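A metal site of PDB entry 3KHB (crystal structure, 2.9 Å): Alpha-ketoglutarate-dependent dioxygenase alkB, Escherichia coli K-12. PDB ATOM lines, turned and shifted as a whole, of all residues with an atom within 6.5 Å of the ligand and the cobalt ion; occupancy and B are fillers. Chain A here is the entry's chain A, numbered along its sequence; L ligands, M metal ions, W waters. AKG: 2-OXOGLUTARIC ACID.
O3 of the ligand lies within hydrogen-bond range of OH of Tyr 125 (2.6 Å). O3 of the ligand lies within salt-bridge range of NH1 of Arg 207. The side-chain amide nitrogen (ND2) of Asn 209 lies within hydrogen-bond range of an oxygen (O4) of the ligand. O1 of the ligand lies within hydrogen-bond range of ND2 of Asn 123. The guanidinium group (NH1) of Arg 213 sits close to an oxygen (O2) of the ligand, at 3.7 Å.
The cobalt ion is bound by a ring nitrogen (NE2) of His 190 (2.1 Å). NE2 of His 134 is bound to the cobalt ion, 2.1 Å away. The cobalt ion is bound by an oxygen (O5) of the ligand. The cobalt ion is bound by the side-chain carboxylate (OD1) of Asp 136, at 2.3 Å. An oxygen (O2) of the ligand binds the cobalt ion (2.3 Å). The cobalt ion has five donor atoms within binding distance.
Water W1 lies within hydrogen-bond range of O4 of the ligand (2.6 Å) and OG of Ser 148 (3.0 Å).
Leu 121 touches the ligand (CD2 to O1, 3.9 Å). CD2 of Leu 131 touches C2 of the ligand (3.5 Å). Ser 148 touches the ligand. Ile 192 touches the ligand (CG1 to O3, 3.5 Å). CG2 of Thr 211 touches O1 of the ligand, 3.4 Å away. Hydrophobic or aromatic side chains that line the ligand: Leu 121, Tyr 125, Leu 131, His 134, His 190 and Ile 192. Within 4 Å of the ligand: Leu 121, Asn 123, Tyr 125, Leu 131, His 134, Asp 136, Ser 148, His 190, Ile 192, Arg 207, Asn 209, Thr 211 and Arg 213. The nearest printed residue that does not touch the ligand is Phe 157 (4.1 Å).
Of the 22 residues printed, 3 come within 4 Å of the cobalt ion.
The side-chain carboxylate (OD2) of Asp 136 lies within salt-bridge range of the guanidinium group (NH1) of Arg 213, at 2.8 Å. The side-chain hydroxyl (OG) of Ser 150 lies within hydrogen-bond range of the guanidinium group (NH2) of Arg 207 (3.1 Å). N of Asn 123 lies within hydrogen-bond range of O of Asn 209, 2.7 Å away. The side-chain hydroxyl (OG) of Ser 148 is in hydrogen-bond range of the side-chain amide nitrogen (ND2) of Asn 209 (3.2 Å). The side-chain amide nitrogen of Asn 209 sits at hydrogen-bond distance from the backbone carbonyl oxygen of Val 149 (2.7 Å). NH2 of Arg 213 is in hydrogen-bond range of OG1 of Thr 211, 3.1 Å away. O of Thr 211 is in hydrogen-bond range of N of Leu 121 (3.1 Å). N of Ile 192 sits at hydrogen-bond distance from O of Leu 131 (2.8 Å).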
ATOM      1  N   LEU A 121      -3.920  16.227 -24.525  1.00  0.00           N
ATOM      2  CA  LEU A 121      -3.731  17.261 -25.543  1.00  0.00           C
ATOM      3  C   LEU A 121      -2.242  17.529 -25.776  1.00  0.00           C
ATOM      4  O   LEU A 121      -1.556  18.086 -24.920  1.00  0.00           O
ATOM      5  CB  LEU A 121      -4.464  18.562 -25.162  1.00  0.00           C
ATOM      6  CG  LEU A 121      -4.256  19.851 -25.969  1.00  0.00           C
ATOM      7  CD1 LEU A 121      -4.667  19.699 -27.434  1.00  0.00           C
ATOM      8  CD2 LEU A 121      -4.989  21.020 -25.338  1.00  0.00           C
ATOM      9  N   ASN A 123       0.771  19.382 -27.525  1.00  0.00           N
ATOM     10  CA  ASN A 123       1.071  20.690 -28.114  1.00  0.00           C
ATOM     11  C   ASN A 123       2.445  20.723 -28.764  1.00  0.00           C
ATOM     12  O   ASN A 123       3.395  20.139 -28.248  1.00  0.00           O
ATOM     13  CB  ASN A 123       1.010  21.783 -27.053  1.00  0.00           C
ATOM     14  CG  ASN A 123      -0.333  21.865 -26.357  1.00  0.00           C
ATOM     15  OD1 ASN A 123      -1.373  21.638 -26.972  1.00  0.00           O
ATOM     16  ND2 ASN A 123      -0.311  22.190 -25.077  1.00  0.00           N
ATOM     17  N   TYR A 125       5.142  23.640 -30.268  1.00  0.00           N
ATOM     18  CA  TYR A 125       5.451  25.068 -30.352  1.00  0.00           C
ATOM     19  C   TYR A 125       6.626  25.346 -31.279  1.00  0.00           C
ATOM     20  O   TYR A 125       7.700  24.759 -31.121  1.00  0.00           O
ATOM     21  CB  TYR A 125       5.811  25.637 -28.977  1.00  0.00           C
ATOM     22  CG  TYR A 125       4.718  25.624 -27.941  1.00  0.00           C
ATOM     23  CD1 TYR A 125       4.354  24.442 -27.290  1.00  0.00           C
ATOM     24  CD2 TYR A 125       4.066  26.811 -27.572  1.00  0.00           C
ATOM     25  CE1 TYR A 125       3.359  24.442 -26.318  1.00  0.00           C
ATOM     26  CE2 TYR A 125       3.078  26.812 -26.608  1.00  0.00           C
ATOM     27  CZ  TYR A 125       2.731  25.622 -25.982  1.00  0.00           C
ATOM     28  OH  TYR A 125       1.755  25.612 -25.022  1.00  0.00           O
ATOM     29  N   LEU A 131       1.212  30.252 -25.783  1.00  0.00           N
ATOM     30  CA  LEU A 131      -0.080  29.970 -25.192  1.00  0.00           C
ATOM     31  C   LEU A 131      -0.496  31.118 -24.266  1.00  0.00           C
ATOM     32  O   LEU A 131       0.182  31.416 -23.276  1.00  0.00           O
ATOM     33  CB  LEU A 131      -0.061  28.647 -24.445  1.00  0.00           C
ATOM     34  CG  LEU A 131      -1.427  28.051 -24.136  1.00  0.00           C
ATOM     35  CD1 LEU A 131      -2.246  27.896 -25.417  1.00  0.00           C
ATOM     36  CD2 LEU A 131      -1.248  26.717 -23.458  1.00  0.00           C
ATOM     37  N   HIS A 134      -4.443  31.391 -19.257  1.00  0.00           N
ATOM     38  CA  HIS A 134      -5.747  30.775 -19.141  1.00  0.00           C
ATOM     39  C   HIS A 134      -5.751  29.961 -17.855  1.00  0.00           C
ATOM     40  O   HIS A 134      -4.717  29.800 -17.203  1.00  0.00           O
ATOM     41  CB  HIS A 134      -5.965  29.832 -20.320  1.00  0.00           C
ATOM     42  CG  HIS A 134      -5.015  28.668 -20.341  1.00  0.00           C
ATOM     43  ND1 HIS A 134      -3.806  28.710 -21.001  1.00  0.00           N
ATOM     44  CD2 HIS A 134      -5.093  27.441 -19.768  1.00  0.00           C
ATOM     45  CE1 HIS A 134      -3.178  27.559 -20.835  1.00  0.00           C
ATOM     46  NE2 HIS A 134      -3.947  26.770 -20.101  1.00  0.00           N
ATOM     47  N   GLN A 135      -6.918  29.422 -17.518  1.00  0.00           N
ATOM     48  CA  GLN A 135      -7.027  28.430 -16.463  1.00  0.00           C
ATOM     49  C   GLN A 135      -7.702  27.207 -17.069  1.00  0.00           C
ATOM     50  O   GLN A 135      -8.700  27.341 -17.759  1.00  0.00           O
ATOM     51  CB  GLN A 135      -7.785  29.028 -15.275  1.00  0.00           C
ATOM     52  CG  GLN A 135      -8.798  30.092 -15.647  1.00  0.00           C
ATOM     53  CD  GLN A 135      -9.662  30.503 -14.467  1.00  0.00           C
ATOM     54  OE1 GLN A 135      -9.296  30.313 -13.315  1.00  0.00           O
ATOM     55  NE2 GLN A 135     -10.831  31.072 -14.772  1.00  0.00           N
ATOM     56  N   ASP A 136      -7.123  26.030 -16.841  1.00  0.00           N
ATOM     57  CA  ASP A 136      -7.729  24.762 -17.276  1.00  0.00           C
ATOM     58  C   ASP A 136      -9.103  24.672 -16.654  1.00  0.00           C
ATOM     59  O   ASP A 136      -9.223  24.428 -15.442  1.00  0.00           O
ATOM     60  CB  ASP A 136      -6.870  23.558 -16.856  1.00  0.00           C
ATOM     61  CG  ASP A 136      -5.818  23.190 -17.892  1.00  0.00           C
ATOM     62  OD1 ASP A 136      -5.667  23.903 -18.904  1.00  0.00           O
ATOM     63  OD2 ASP A 136      -5.131  22.174 -17.696  1.00  0.00           O
ATOM     64  N   ILE A 146      -3.746  18.300 -13.090  1.00  0.00           N
ATOM     65  CA  ILE A 146      -3.236  18.452 -14.445  1.00  0.00           C
ATOM     66  C   ILE A 146      -1.764  18.076 -14.435  1.00  0.00           C
ATOM     67  O   ILE A 146      -0.991  18.562 -13.608  1.00  0.00           O
ATOM     68  CB  ILE A 146      -3.351  19.904 -14.966  1.00  0.00           C
ATOM     69  CG1 ILE A 146      -4.713  20.526 -14.636  1.00  0.00           C
ATOM     70  CG2 ILE A 146      -3.074  19.954 -16.465  1.00  0.00           C
ATOM     71  CD1 ILE A 146      -5.845  20.044 -15.516  1.00  0.00           C
ATOM     72  N   SER A 148       1.473  18.281 -16.822  1.00  0.00           N
ATOM     73  CA  SER A 148       2.046  18.893 -18.004  1.00  0.00           C
ATOM     74  C   SER A 148       3.478  18.401 -18.184  1.00  0.00           C
ATOM     75  O   SER A 148       4.276  18.468 -17.250  1.00  0.00           O
ATOM     76  CB  SER A 148       2.004  20.413 -17.879  1.00  0.00           C
ATOM     77  OG  SER A 148       1.997  21.034 -19.152  1.00  0.00           O
ATOM     78  N   VAL A 149       3.801  17.896 -19.373  1.00  0.00           N
ATOM     79  CA  VAL A 149       5.156  17.455 -19.693  1.00  0.00           C
ATOM     80  C   VAL A 149       5.790  18.433 -20.685  1.00  0.00           C
ATOM     81  O   VAL A 149       5.163  18.807 -21.666  1.00  0.00           O
ATOM     82  CB  VAL A 149       5.170  16.025 -20.293  1.00  0.00           C
ATOM     83  CG1 VAL A 149       6.597  15.510 -20.453  1.00  0.00           C
ATOM     84  CG2 VAL A 149       4.342  15.063 -19.442  1.00  0.00           C
ATOM     85  N   SER A 150       7.032  18.824 -20.417  1.00  0.00           N
ATOM     86  CA  SER A 150       7.758  19.760 -21.270  1.00  0.00           C
ATOM     87  C   SER A 150       8.817  18.997 -22.049  1.00  0.00           C
ATOM     88  O   SER A 150       9.648  18.318 -21.455  1.00  0.00           O
ATOM     89  CB  SER A 150       8.445  20.832 -20.419  1.00  0.00           C
ATOM     90  OG  SER A 150       7.596  21.270 -19.376  1.00  0.00           O
ATOM     91  N   PHE A 157       7.223  29.265 -18.535  1.00  0.00           N
ATOM     92  CA  PHE A 157       5.859  28.904 -18.167  1.00  0.00           C
ATOM     93  C   PHE A 157       5.402  29.717 -16.975  1.00  0.00           C
ATOM     94  O   PHE A 157       5.899  29.536 -15.862  1.00  0.00           O
ATOM     95  CB  PHE A 157       5.826  27.415 -17.859  1.00  0.00           C
ATOM     96  CG  PHE A 157       4.546  26.943 -17.201  1.00  0.00           C
ATOM     97  CD1 PHE A 157       3.370  26.819 -17.933  1.00  0.00           C
ATOM     98  CD2 PHE A 157       4.549  26.546 -15.861  1.00  0.00           C
ATOM     99  CE1 PHE A 157       2.204  26.347 -17.328  1.00  0.00           C
ATOM    100  CE2 PHE A 157       3.391  26.074 -15.251  1.00  0.00           C
ATOM    101  CZ  PHE A 157       2.215  25.979 -15.979  1.00  0.00           C
ATOM    102  N   LEU A 173      10.898  25.978 -17.969  1.00  0.00           N
ATOM    103  CA  LEU A 173      10.612  24.562 -18.154  1.00  0.00           C
ATOM    104  C   LEU A 173      11.504  24.041 -19.272  1.00  0.00           C
ATOM    105  O   LEU A 173      11.490  24.552 -20.386  1.00  0.00           O
ATOM    106  CB  LEU A 173       9.136  24.312 -18.483  1.00  0.00           C
ATOM    107  CG  LEU A 173       8.041  24.761 -17.509  1.00  0.00           C
ATOM    108  CD1 LEU A 173       6.740  24.057 -17.822  1.00  0.00           C
ATOM    109  CD2 LEU A 173       8.405  24.563 -16.046  1.00  0.00           C
ATOM    110  N   TRP A 181      -0.294  20.124 -11.260  1.00  0.00           N
ATOM    111  CA  TRP A 181      -1.055  21.023 -10.386  1.00  0.00           C
ATOM    112  C   TRP A 181      -2.529  20.630 -10.215  1.00  0.00           C
ATOM    113  O   TRP A 181      -3.226  20.341 -11.193  1.00  0.00           O
ATOM    114  CB  TRP A 181      -0.887  22.507 -10.794  1.00  0.00           C
ATOM    115  CG  TRP A 181      -1.623  22.937 -12.026  1.00  0.00           C
ATOM    116  CD1 TRP A 181      -2.838  23.549 -12.087  1.00  0.00           C
ATOM    117  CD2 TRP A 181      -1.172  22.820 -13.386  1.00  0.00           C
ATOM    118  NE1 TRP A 181      -3.183  23.808 -13.393  1.00  0.00           N
ATOM    119  CE2 TRP A 181      -2.178  23.364 -14.208  1.00  0.00           C
ATOM    120  CE3 TRP A 181      -0.013  22.292 -13.983  1.00  0.00           C
ATOM    121  CZ2 TRP A 181      -2.064  23.400 -15.605  1.00  0.00           C
ATOM    122  CZ3 TRP A 181       0.095  22.327 -15.372  1.00  0.00           C
ATOM    123  CH2 TRP A 181      -0.920  22.878 -16.163  1.00  0.00           C
ATOM    124  N   HIS A 190      -2.284  30.055 -15.828  1.00  0.00           N
ATOM    125  CA  HIS A 190      -0.962  29.631 -16.270  1.00  0.00           C
ATOM    126  C   HIS A 190      -0.881  29.853 -17.775  1.00  0.00           C
ATOM    127  O   HIS A 190      -1.904  30.083 -18.412  1.00  0.00           O
ATOM    128  CB  HIS A 190      -0.713  28.146 -15.939  1.00  0.00           C
ATOM    129  CG  HIS A 190      -1.698  27.223 -16.574  1.00  0.00           C
ATOM    130  ND1 HIS A 190      -3.016  27.135 -16.149  1.00  0.00           N
ATOM    131  CD2 HIS A 190      -1.577  26.378 -17.619  1.00  0.00           C
ATOM    132  CE1 HIS A 190      -3.654  26.261 -16.909  1.00  0.00           C
ATOM    133  NE2 HIS A 190      -2.805  25.785 -17.806  1.00  0.00           N
ATOM    134  N   GLY A 191       0.318  29.793 -18.339  1.00  0.00           N
ATOM    135  CA  GLY A 191       0.470  30.042 -19.764  1.00  0.00           C
ATOM    136  C   GLY A 191       1.897  29.949 -20.237  1.00  0.00           C
ATOM    137  O   GLY A 191       2.784  29.559 -19.477  1.00  0.00           O
ATOM    138  N   ILE A 192       2.121  30.325 -21.498  1.00  0.00           N
ATOM    139  CA  ILE A 192       3.440  30.180 -22.156  1.00  0.00           C
ATOM    140  C   ILE A 192       3.832  31.434 -22.917  1.00  0.00           C
ATOM    141  O   ILE A 192       3.018  31.999 -23.657  1.00  0.00           O
ATOM    142  CB  ILE A 192       3.480  28.930 -23.082  1.00  0.00           C
ATOM    143  CG1 ILE A 192       3.419  27.631 -22.255  1.00  0.00           C
ATOM    144  CG2 ILE A 192       4.714  28.931 -23.990  1.00  0.00           C
ATOM    145  CD1 ILE A 192       4.621  27.372 -21.374  1.00  0.00           C
ATOM    146  N   ARG A 207       9.266  22.825 -29.555  1.00  0.00           N
ATOM    147  CA  ARG A 207       8.960  22.274 -28.233  1.00  0.00           C
ATOM    148  C   ARG A 207       7.650  21.484 -28.261  1.00  0.00           C
ATOM    149  O   ARG A 207       6.618  21.992 -28.695  1.00  0.00           O
ATOM    150  CB  ARG A 207       8.870  23.379 -27.181  1.00  0.00           C
ATOM    151  CG  ARG A 207       8.266  22.913 -25.860  1.00  0.00           C
ATOM    152  CD  ARG A 207       7.788  24.074 -25.016  1.00  0.00           C
ATOM    153  NE  ARG A 207       7.747  23.719 -23.592  1.00  0.00           N
ATOM    154  CZ  ARG A 207       6.648  23.653 -22.865  1.00  0.00           C
ATOM    155  NH1 ARG A 207       5.456  23.919 -23.401  1.00  0.00           N
ATOM    156  NH2 ARG A 207       6.728  23.320 -21.587  1.00  0.00           N
ATOM    157  N   ASN A 209       4.769  19.453 -25.856  1.00  0.00           N
ATOM    158  CA  ASN A 209       4.214  19.537 -24.513  1.00  0.00           C
ATOM    159  C   ASN A 209       2.972  18.668 -24.411  1.00  0.00           C
ATOM    160  O   ASN A 209       2.041  18.839 -25.185  1.00  0.00           O
ATOM    161  CB  ASN A 209       3.897  20.992 -24.160  1.00  0.00           C
ATOM    162  CG  ASN A 209       3.137  21.121 -22.853  1.00  0.00           C
ATOM    163  OD1 ASN A 209       1.902  21.222 -22.848  1.00  0.00           O
ATOM    164  ND2 ASN A 209       3.854  21.120 -21.736  1.00  0.00           N
ATOM    165  N   LEU A 210       2.968  17.735 -23.472  1.00  0.00           N
ATOM    166  CA  LEU A 210       1.785  16.927 -23.233  1.00  0.00           C
ATOM    167  C   LEU A 210       1.068  17.436 -21.998  1.00  0.00           C
ATOM    168  O   LEU A 210       1.714  17.650 -20.965  1.00  0.00           O
ATOM    169  CB  LEU A 210       2.137  15.442 -23.026  1.00  0.00           C
ATOM    170  CG  LEU A 210       3.253  14.779 -23.829  1.00  0.00           C
ATOM    171  CD1 LEU A 210       3.611  13.429 -23.244  1.00  0.00           C
ATOM    172  CD2 LEU A 210       2.886  14.655 -25.296  1.00  0.00           C
ATOM    173  N   THR A 211      -0.236  17.653 -22.097  1.00  0.00           N
ATOM    174  CA  THR A 211      -1.060  17.858 -20.893  1.00  0.00           C
ATOM    175  C   THR A 211      -2.052  16.708 -20.742  1.00  0.00           C
ATOM    176  O   THR A 211      -2.877  16.454 -21.624  1.00  0.00           O
ATOM    177  CB  THR A 211      -1.775  19.237 -20.829  1.00  0.00           C
ATOM    178  OG1 THR A 211      -2.805  19.308 -21.811  1.00  0.00           O
ATOM    179  CG2 THR A 211      -0.789  20.383 -21.023  1.00  0.00           C
ATOM    180  N   ARG A 213      -5.160  14.852 -18.677  1.00  0.00           N
ATOM    181  CA  ARG A 213      -6.373  15.312 -18.001  1.00  0.00           C
ATOM    182  C   ARG A 213      -7.430  14.228 -17.867  1.00  0.00           C
ATOM    183  O   ARG A 213      -7.516  13.327 -18.708  1.00  0.00           O
ATOM    184  CB  ARG A 213      -6.970  16.540 -18.724  1.00  0.00           C
ATOM    185  CG  ARG A 213      -6.283  17.862 -18.424  1.00  0.00           C
ATOM    186  CD  ARG A 213      -7.062  19.057 -18.972  1.00  0.00           C
ATOM    187  NE  ARG A 213      -6.817  19.281 -20.393  1.00  0.00           N
ATOM    188  CZ  ARG A 213      -5.882  20.093 -20.890  1.00  0.00           C
ATOM    189  NH1 ARG A 213      -5.070  20.770 -20.081  1.00  0.00           N
ATOM    190  NH2 ARG A 213      -5.750  20.216 -22.192  1.00  0.00           N
HETATM  191  C1  AKG L   1      -2.569  23.488 -21.935  1.00  0.00           C
HETATM  192  O1  AKG L   1      -2.413  22.701 -22.898  1.00  0.00           O
HETATM  193  O2  AKG L   1      -3.710  23.861 -21.562  1.00  0.00           O
HETATM  194  C2  AKG L   1      -1.392  24.009 -21.230  1.00  0.00           C
HETATM  195  O5  AKG L   1      -1.561  24.692 -20.235  1.00  0.00           O
HETATM  196  C3  AKG L   1      -0.005  23.679 -21.727  1.00  0.00           C
HETATM  197  C4  AKG L   1       1.032  24.715 -21.294  1.00  0.00           C
HETATM  198  C5  AKG L   1       2.420  24.306 -21.723  1.00  0.00           C
HETATM  199  O3  AKG L   1       2.703  24.311 -22.948  1.00  0.00           O
HETATM  200  O4  AKG L   1       3.255  23.985 -20.846  1.00  0.00           O
HETATM  201 CO    CO M   1      -3.627  24.778 -19.451  1.00  0.00          CO
HETATM  202  O   HOH W   1       3.412  23.575 -18.320  1.00  0.00           O
HETATM  203  O   HOH W   2      -5.693  24.440 -24.079  1.00  0.00           O
